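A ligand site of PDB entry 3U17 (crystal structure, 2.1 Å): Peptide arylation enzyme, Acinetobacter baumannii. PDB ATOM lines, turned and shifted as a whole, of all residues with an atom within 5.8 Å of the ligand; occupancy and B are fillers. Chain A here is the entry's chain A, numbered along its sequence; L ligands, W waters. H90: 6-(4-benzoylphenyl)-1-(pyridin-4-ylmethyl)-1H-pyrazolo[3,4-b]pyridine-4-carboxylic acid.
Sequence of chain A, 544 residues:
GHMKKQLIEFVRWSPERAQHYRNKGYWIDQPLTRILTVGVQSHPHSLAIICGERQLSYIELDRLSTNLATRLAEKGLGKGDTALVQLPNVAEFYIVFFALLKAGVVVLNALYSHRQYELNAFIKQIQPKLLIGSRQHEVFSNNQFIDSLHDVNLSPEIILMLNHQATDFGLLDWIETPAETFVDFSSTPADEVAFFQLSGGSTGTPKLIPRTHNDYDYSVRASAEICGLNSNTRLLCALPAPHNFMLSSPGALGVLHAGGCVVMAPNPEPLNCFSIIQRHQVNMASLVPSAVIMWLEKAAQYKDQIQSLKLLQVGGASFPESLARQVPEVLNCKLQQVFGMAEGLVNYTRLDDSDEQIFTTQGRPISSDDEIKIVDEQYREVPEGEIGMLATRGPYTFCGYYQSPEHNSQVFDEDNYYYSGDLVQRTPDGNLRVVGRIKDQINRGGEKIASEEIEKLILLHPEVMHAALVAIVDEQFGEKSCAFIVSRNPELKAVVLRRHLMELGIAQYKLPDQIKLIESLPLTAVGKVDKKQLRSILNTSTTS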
ATOM      1  N   LEU A 111      30.925  -1.295 -10.212  1.00  0.00           N
ATOM      2  CA  LEU A 111      31.141  -1.451 -11.633  1.00  0.00           C
ATOM      3  C   LEU A 111      32.340  -2.374 -11.840  1.00  0.00           C
ATOM      4  O   LEU A 111      33.345  -2.265 -11.133  1.00  0.00           O
ATOM      5  CB  LEU A 111      31.376  -0.104 -12.307  1.00  0.00           C
ATOM      6  CG  LEU A 111      30.241   0.919 -12.189  1.00  0.00           C
ATOM      7  CD1 LEU A 111      30.646   2.267 -12.784  1.00  0.00           C
ATOM      8  CD2 LEU A 111      28.949   0.401 -12.829  1.00  0.00           C
ATOM      9  N   SER A 113      34.392  -2.128 -14.057  1.00  0.00           N
ATOM     10  CA  SER A 113      35.511  -1.251 -14.402  1.00  0.00           C
ATOM     11  C   SER A 113      36.113  -0.553 -13.178  1.00  0.00           C
ATOM     12  O   SER A 113      37.092   0.196 -13.302  1.00  0.00           O
ATOM     13  CB  SER A 113      35.099  -0.202 -15.443  1.00  0.00           C
ATOM     14  OG  SER A 113      34.085   0.664 -14.937  1.00  0.00           O
ATOM     15  N   LEU A 239      25.217  -1.465 -21.716  1.00  0.00           N
ATOM     16  CA  LEU A 239      25.831  -0.574 -20.730  1.00  0.00           C
ATOM     17  C   LEU A 239      26.085  -1.424 -19.488  1.00  0.00           C
ATOM     18  O   LEU A 239      25.572  -2.526 -19.399  1.00  0.00           O
ATOM     19  CB  LEU A 239      24.919   0.616 -20.411  1.00  0.00           C
ATOM     20  CG  LEU A 239      24.476   1.519 -21.573  1.00  0.00           C
ATOM     21  CD1 LEU A 239      23.577   2.649 -21.078  1.00  0.00           C
ATOM     22  CD2 LEU A 239      25.704   2.086 -22.276  1.00  0.00           C
ATOM     23  N   PRO A 240      26.879  -0.931 -18.523  1.00  0.00           N
ATOM     24  CA  PRO A 240      27.137  -1.747 -17.327  1.00  0.00           C
ATOM     25  C   PRO A 240      25.845  -2.086 -16.580  1.00  0.00           C
ATOM     26  O   PRO A 240      25.098  -1.190 -16.189  1.00  0.00           O
ATOM     27  CB  PRO A 240      28.042  -0.855 -16.479  1.00  0.00           C
ATOM     28  CG  PRO A 240      28.727   0.063 -17.491  1.00  0.00           C
ATOM     29  CD  PRO A 240      27.678   0.315 -18.535  1.00  0.00           C
ATOM     30  N   HIS A 243      24.540  -0.072 -13.569  1.00  0.00           N
ATOM     31  CA  HIS A 243      24.264   1.357 -13.701  1.00  0.00           C
ATOM     32  C   HIS A 243      22.767   1.658 -13.608  1.00  0.00           C
ATOM     33  O   HIS A 243      21.948   0.944 -14.198  1.00  0.00           O
ATOM     34  CB  HIS A 243      24.823   1.919 -15.021  1.00  0.00           C
ATOM     35  CG  HIS A 243      24.895   3.414 -15.021  1.00  0.00           C
ATOM     36  ND1 HIS A 243      23.778   4.204 -15.180  1.00  0.00           N
ATOM     37  CD2 HIS A 243      25.937   4.254 -14.790  1.00  0.00           C
ATOM     38  CE1 HIS A 243      24.135   5.475 -15.080  1.00  0.00           C
ATOM     39  NE2 HIS A 243      25.441   5.528 -14.851  1.00  0.00           N
ATOM     40  N   ASN A 244      22.424   2.708 -12.868  1.00  0.00           N
ATOM     41  CA  ASN A 244      21.016   3.047 -12.653  1.00  0.00           C
ATOM     42  C   ASN A 244      20.231   3.102 -13.968  1.00  0.00           C
ATOM     43  O   ASN A 244      19.080   2.652 -14.038  1.00  0.00           O
ATOM     44  CB  ASN A 244      20.893   4.373 -11.896  1.00  0.00           C
ATOM     45  CG  ASN A 244      19.527   4.555 -11.242  1.00  0.00           C
ATOM     46  OD1 ASN A 244      19.097   3.733 -10.413  1.00  0.00           O
ATOM     47  ND2 ASN A 244      18.828   5.620 -11.617  1.00  0.00           N
ATOM     48  N   PHE A 245      20.861   3.635 -15.015  1.00  0.00           N
ATOM     49  CA  PHE A 245      20.276   3.725 -16.345  1.00  0.00           C
ATOM     50  C   PHE A 245      19.947   2.327 -16.873  1.00  0.00           C
ATOM     51  O   PHE A 245      18.804   2.070 -17.275  1.00  0.00           O
ATOM     52  CB  PHE A 245      21.252   4.452 -17.288  1.00  0.00           C
ATOM     53  CG  PHE A 245      20.688   4.781 -18.668  1.00  0.00           C
ATOM     54  CD1 PHE A 245      19.327   4.725 -18.924  1.00  0.00           C
ATOM     55  CD2 PHE A 245      21.553   5.170 -19.702  1.00  0.00           C
ATOM     56  CE1 PHE A 245      18.816   5.047 -20.191  1.00  0.00           C
ATOM     57  CE2 PHE A 245      21.055   5.497 -20.970  1.00  0.00           C
ATOM     58  CZ  PHE A 245      19.676   5.432 -21.217  1.00  0.00           C
ATOM     59  N   SER A 248      17.370   0.193 -14.141  1.00  0.00           N
ATOM     60  CA  SER A 248      16.031   0.599 -13.737  1.00  0.00           C
ATOM     61  C   SER A 248      15.356   1.663 -14.612  1.00  0.00           C
ATOM     62  O   SER A 248      14.243   2.097 -14.287  1.00  0.00           O
ATOM     63  CB  SER A 248      16.076   1.137 -12.310  1.00  0.00           C
ATOM     64  OG  SER A 248      16.715   2.397 -12.270  1.00  0.00           O
ATOM     65  N   SER A 249      15.987   2.086 -15.700  1.00  0.00           N
ATOM     66  CA  SER A 249      15.434   3.248 -16.426  1.00  0.00           C
ATOM     67  C   SER A 249      15.129   3.089 -17.923  1.00  0.00           C
ATOM     68  O   SER A 249      15.634   3.867 -18.722  1.00  0.00           O
ATOM     69  CB  SER A 249      16.318   4.479 -16.201  1.00  0.00           C
ATOM     70  OG  SER A 249      16.423   4.763 -14.807  1.00  0.00           O
ATOM     71  N   VAL A 288      24.664   5.632 -24.293  1.00  0.00           N
ATOM     72  CA  VAL A 288      25.126   6.985 -24.051  1.00  0.00           C
ATOM     73  C   VAL A 288      25.554   7.554 -25.420  1.00  0.00           C
ATOM     74  O   VAL A 288      25.801   6.786 -26.349  1.00  0.00           O
ATOM     75  CB  VAL A 288      26.298   7.008 -23.046  1.00  0.00           C
ATOM     76  CG1 VAL A 288      25.831   6.459 -21.682  1.00  0.00           C
ATOM     77  CG2 VAL A 288      27.495   6.210 -23.588  1.00  0.00           C
ATOM     78  N   GLY A 315      20.921   8.581 -23.061  1.00  0.00           N
ATOM     79  CA  GLY A 315      21.147   9.481 -21.945  1.00  0.00           C
ATOM     80  C   GLY A 315      22.612   9.658 -21.621  1.00  0.00           C
ATOM     81  O   GLY A 315      23.458   8.828 -21.990  1.00  0.00           O
ATOM     82  N   GLY A 316      22.916  10.744 -20.925  1.00  0.00           N
ATOM     83  CA  GLY A 316      24.278  11.014 -20.508  1.00  0.00           C
ATOM     84  C   GLY A 316      24.882  12.123 -21.348  1.00  0.00           C
ATOM     85  O   GLY A 316      24.278  12.560 -22.330  1.00  0.00           O
ATOM     86  N   ALA A 317      26.063  12.584 -20.960  1.00  0.00           N
ATOM     87  CA  ALA A 317      26.777  13.584 -21.766  1.00  0.00           C
ATOM     88  C   ALA A 317      25.889  14.683 -22.349  1.00  0.00           C
ATOM     89  O   ALA A 317      25.160  15.388 -21.644  1.00  0.00           O
ATOM     90  CB  ALA A 317      27.574  12.898 -22.902  1.00  0.00           C
ATOM     91  N   VAL A 338      16.659  10.423 -22.184  1.00  0.00           N
ATOM     92  CA  VAL A 338      16.561  10.153 -20.764  1.00  0.00           C
ATOM     93  C   VAL A 338      17.603  10.973 -20.041  1.00  0.00           C
ATOM     94  O   VAL A 338      18.788  10.894 -20.360  1.00  0.00           O
ATOM     95  CB  VAL A 338      16.854   8.668 -20.463  1.00  0.00           C
ATOM     96  CG1 VAL A 338      16.628   8.354 -18.969  1.00  0.00           C
ATOM     97  CG2 VAL A 338      16.007   7.775 -21.350  1.00  0.00           C
ATOM     98  N   PHE A 339      17.146  11.775 -19.084  1.00  0.00           N
ATOM     99  CA  PHE A 339      18.049  12.441 -18.166  1.00  0.00           C
ATOM    100  C   PHE A 339      17.670  12.017 -16.730  1.00  0.00           C
ATOM    101  O   PHE A 339      16.617  12.374 -16.218  1.00  0.00           O
ATOM    102  CB  PHE A 339      17.987  13.965 -18.312  1.00  0.00           C
ATOM    103  CG  PHE A 339      18.757  14.678 -17.253  1.00  0.00           C
ATOM    104  CD1 PHE A 339      20.140  14.600 -17.222  1.00  0.00           C
ATOM    105  CD2 PHE A 339      18.111  15.367 -16.260  1.00  0.00           C
ATOM    106  CE1 PHE A 339      20.858  15.232 -16.226  1.00  0.00           C
ATOM    107  CE2 PHE A 339      18.817  15.995 -15.263  1.00  0.00           C
ATOM    108  CZ  PHE A 339      20.191  15.937 -15.241  1.00  0.00           C
ATOM    109  N   GLY A 340      18.541  11.241 -16.102  1.00  0.00           N
ATOM    110  CA  GLY A 340      18.267  10.711 -14.790  1.00  0.00           C
ATOM    111  C   GLY A 340      19.497  10.765 -13.914  1.00  0.00           C
ATOM    112  O   GLY A 340      20.540  11.279 -14.324  1.00  0.00           O
ATOM    113  N   MET A 341      19.372  10.218 -12.705  1.00  0.00           N
ATOM    114  CA  MET A 341      20.488  10.192 -11.764  1.00  0.00           C
ATOM    115  C   MET A 341      20.284   9.058 -10.788  1.00  0.00           C
ATOM    116  O   MET A 341      19.149   8.739 -10.423  1.00  0.00           O
ATOM    117  CB  MET A 341      20.617  11.532 -11.035  1.00  0.00           C
ATOM    118  CG  MET A 341      19.364  11.953 -10.287  1.00  0.00           C
ATOM    119  SD  MET A 341      19.337  13.699  -9.846  1.00  0.00           S
ATOM    120  CE  MET A 341      19.282  14.445 -11.477  1.00  0.00           C
ATOM    121  N   ALA A 342      21.382   8.413 -10.397  1.00  0.00           N
ATOM    122  CA  ALA A 342      21.324   7.308  -9.450  1.00  0.00           C
ATOM    123  C   ALA A 342      20.691   7.734  -8.119  1.00  0.00           C
ATOM    124  O   ALA A 342      20.144   6.905  -7.401  1.00  0.00           O
ATOM    125  CB  ALA A 342      22.710   6.723  -9.223  1.00  0.00           C
ATOM    126  N   GLY A 344      18.032   9.403  -7.791  1.00  0.00           N
ATOM    127  CA  GLY A 344      16.578   9.337  -7.879  1.00  0.00           C
ATOM    128  C   GLY A 344      15.981   9.781  -9.196  1.00  0.00           C
ATOM    129  O   GLY A 344      15.903   8.996 -10.150  1.00  0.00           O
ATOM    130  N   LEU A 345      15.567  11.062  -9.249  1.00  0.00           N
ATOM    131  CA  LEU A 345      14.869  11.649 -10.407  1.00  0.00           C
ATOM    132  C   LEU A 345      15.326  11.155 -11.777  1.00  0.00           C
ATOM    133  O   LEU A 345      16.507  11.247 -12.132  1.00  0.00           O
ATOM    134  CB  LEU A 345      15.006  13.177 -10.398  1.00  0.00           C
ATOM    135  CG  LEU A 345      14.407  13.902 -11.615  1.00  0.00           C
ATOM    136  CD1 LEU A 345      12.892  13.788 -11.598  1.00  0.00           C
ATOM    137  CD2 LEU A 345      14.818  15.376 -11.679  1.00  0.00           C
ATOM    138  N   VAL A 346      14.369  10.692 -12.576  1.00  0.00           N
ATOM    139  CA  VAL A 346      14.605  10.326 -13.958  1.00  0.00           C
ATOM    140  C   VAL A 346      13.574  10.995 -14.845  1.00  0.00           C
ATOM    141  O   VAL A 346      12.378  11.005 -14.528  1.00  0.00           O
ATOM    142  CB  VAL A 346      14.535   8.801 -14.196  1.00  0.00           C
ATOM    143  CG1 VAL A 346      14.919   8.485 -15.646  1.00  0.00           C
ATOM    144  CG2 VAL A 346      15.438   8.053 -13.227  1.00  0.00           C
ATOM    145  N   ASP A 422      23.064  20.043 -11.706  1.00  0.00           N
ATOM    146  CA  ASP A 422      22.723  20.189 -13.114  1.00  0.00           C
ATOM    147  C   ASP A 422      22.117  21.556 -13.416  1.00  0.00           C
ATOM    148  O   ASP A 422      21.378  22.103 -12.613  1.00  0.00           O
ATOM    149  CB  ASP A 422      21.756  19.092 -13.527  1.00  0.00           C
ATOM    150  CG  ASP A 422      22.342  17.724 -13.345  1.00  0.00           C
ATOM    151  OD1 ASP A 422      21.782  16.928 -12.553  1.00  0.00           O
ATOM    152  OD2 ASP A 422      23.390  17.447 -13.966  1.00  0.00           O
ATOM    153  N   ARG A 437      26.407  21.911 -16.137  1.00  0.00           N
ATOM    154  CA  ARG A 437      26.587  21.362 -14.807  1.00  0.00           C
ATOM    155  C   ARG A 437      27.410  22.352 -13.994  1.00  0.00           C
ATOM    156  O   ARG A 437      28.314  22.994 -14.517  1.00  0.00           O
ATOM    157  CB  ARG A 437      27.284  20.011 -14.883  1.00  0.00           C
ATOM    158  CG  ARG A 437      27.221  19.181 -13.588  1.00  0.00           C
ATOM    159  CD  ARG A 437      27.507  17.697 -13.847  1.00  0.00           C
ATOM    160  NE  ARG A 437      26.300  16.961 -14.220  1.00  0.00           N
ATOM    161  CZ  ARG A 437      26.271  15.784 -14.835  1.00  0.00           C
ATOM    162  NH1 ARG A 437      27.411  15.180 -15.187  1.00  0.00           N
ATOM    163  NH2 ARG A 437      25.103  15.203 -15.115  1.00  0.00           N
HETATM  164  C1  H90 L   1      20.819   7.731 -14.256  1.00  0.00           C
HETATM  165  C2  H90 L   1      21.120   8.240 -15.533  1.00  0.00           C
HETATM  166  C3  H90 L   1      20.261   8.047 -16.616  1.00  0.00           C
HETATM  167  C4  H90 L   1      19.090   7.335 -16.357  1.00  0.00           C
HETATM  168  C5  H90 L   1      18.825   6.835 -15.063  1.00  0.00           C
HETATM  169  N6  H90 L   1      19.676   7.051 -14.040  1.00  0.00           N
HETATM  170  C7  H90 L   1      20.613   8.605 -18.017  1.00  0.00           C
HETATM  171  N8  H90 L   1      21.662   9.592 -17.747  1.00  0.00           N
HETATM  172  C9  H90 L   1      22.973   9.455 -17.677  1.00  0.00           C
HETATM  173  C10 H90 L   1      23.428  10.709 -17.306  1.00  0.00           C
HETATM  174  C11 H90 L   1      22.330  11.630 -17.161  1.00  0.00           C
HETATM  175  N12 H90 L   1      21.238  10.895 -17.452  1.00  0.00           N
HETATM  176  N13 H90 L   1      23.791   8.398 -17.876  1.00  0.00           N
HETATM  177  C14 H90 L   1      25.107   8.544 -17.698  1.00  0.00           C
HETATM  178  C15 H90 L   1      25.655   9.786 -17.360  1.00  0.00           C
HETATM  179  C16 H90 L   1      24.807  10.884 -17.149  1.00  0.00           C
HETATM  180  C18 H90 L   1      25.365  12.228 -16.766  1.00  0.00           C
HETATM  181  O19 H90 L   1      24.574  13.177 -16.576  1.00  0.00           O
HETATM  182  O20 H90 L   1      26.588  12.383 -16.636  1.00  0.00           O
HETATM  183  C21 H90 L   1      25.926   7.357 -17.949  1.00  0.00           C
HETATM  184  C22 H90 L   1      25.290   6.149 -18.200  1.00  0.00           C
HETATM  185  C23 H90 L   1      26.053   5.020 -18.460  1.00  0.00           C
HETATM  186  C24 H90 L   1      27.452   5.106 -18.453  1.00  0.00           C
HETATM  187  C25 H90 L   1      28.065   6.330 -18.210  1.00  0.00           C
HETATM  188  C26 H90 L   1      27.302   7.459 -17.950  1.00  0.00           C
HETATM  189  C27 H90 L   1      28.291   3.908 -18.761  1.00  0.00           C
HETATM  190  O27 H90 L   1      28.014   3.216 -19.728  1.00  0.00           O
HETATM  191  C28 H90 L   1      29.517   3.572 -17.952  1.00  0.00           C
HETATM  192  C29 H90 L   1      30.497   2.754 -18.524  1.00  0.00           C
HETATM  193  C30 H90 L   1      31.654   2.429 -17.825  1.00  0.00           C
HETATM  194  C31 H90 L   1      31.816   2.923 -16.536  1.00  0.00           C
HETATM  195  C32 H90 L   1      30.844   3.736 -15.973  1.00  0.00           C
HETATM  196  C33 H90 L   1      29.688   4.061 -16.673  1.00  0.00           C
HETATM  197  O   HOH W   1      23.116  12.650 -13.807  1.00  0.00           O
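N12 of the ligand is in hydrogen-bond range of N of Gly 340 (3.0 Å). ND2 of Asn 244 is in hydrogen-bond range of N6 of the ligand. N of Met 341 sits close to N6 of the ligand (3.5 Å). An oxygen (O19) of the ligand lies within salt-bridge range of the guanidinium group (NH2) of Arg 437.
The backbone carbonyl oxygen of Asn 244 sits at hydrogen-bond distance from the side-chain hydroxyl of Ser 249 (3.5 Å). O of Met 341 is in hydrogen-bond range of ND2 of Asn 244, at 3.4 Å. The side-chain carboxylate of Asp 422 lies within salt-bridge range of the guanidinium group of Arg 437 (3.0 Å). The backbone NH (N) of Phe 245 is in hydrogen-bond range of a ring nitrogen (ND1) of His 243 (3.0 Å). The backbone carbonyl oxygen (O) of Asn 244 is in hydrogen-bond range of the side-chain hydroxyl (OG) of Ser 248, 3.0 Å away. OG of Ser 248 sits close to OG of Ser 249, 3.5 Å away.
Leu 111 touches the ligand. Ser 113 touches the ligand. Leu 239 touches the ligand (CD2 to O27, 3.6 Å). CD of Pro 240 touches O27 of the ligand, 3.2 Å away. His 243 touches the ligand (CE1 to C22, 3.4 Å). Phe 245 touches the ligand. OG of Ser 249 touches C5 of the ligand (3.2 Å). Val 288 touches the ligand (CG1 to C23, 3.5 Å). C of Gly 315 touches C9 of the ligand (3.97 Å). Gly 316 touches the ligand. CG1 of Val 338 touches C4 of the ligand, 3.7 Å away. Phe 339 touches the ligand (CA to N12, 3.6 Å). Ala 342 touches the ligand. 17 residues have an atom within 4 Å of the ligand: Leu 111, Ser 113, Leu 239, Pro 240, His 243, Asn 244, Phe 245, Ser 249, Val 288, Gly 315, Gly 316, Val 338, Phe 339, Gly 340, Met 341, Ala 342 and Arg 437. Along chain A the residues within 4 Å of the ligand span positions 111 to 437. The nearest printed residue that does not touch the ligand is Val 346 (4.04 Å).
Water W1 lies within hydrogen-bond range of the backbone carbonyl oxygen (O) of Gly 340, an oxygen (O19) of the ligand and the guanidinium group (NH2) of Arg 437.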
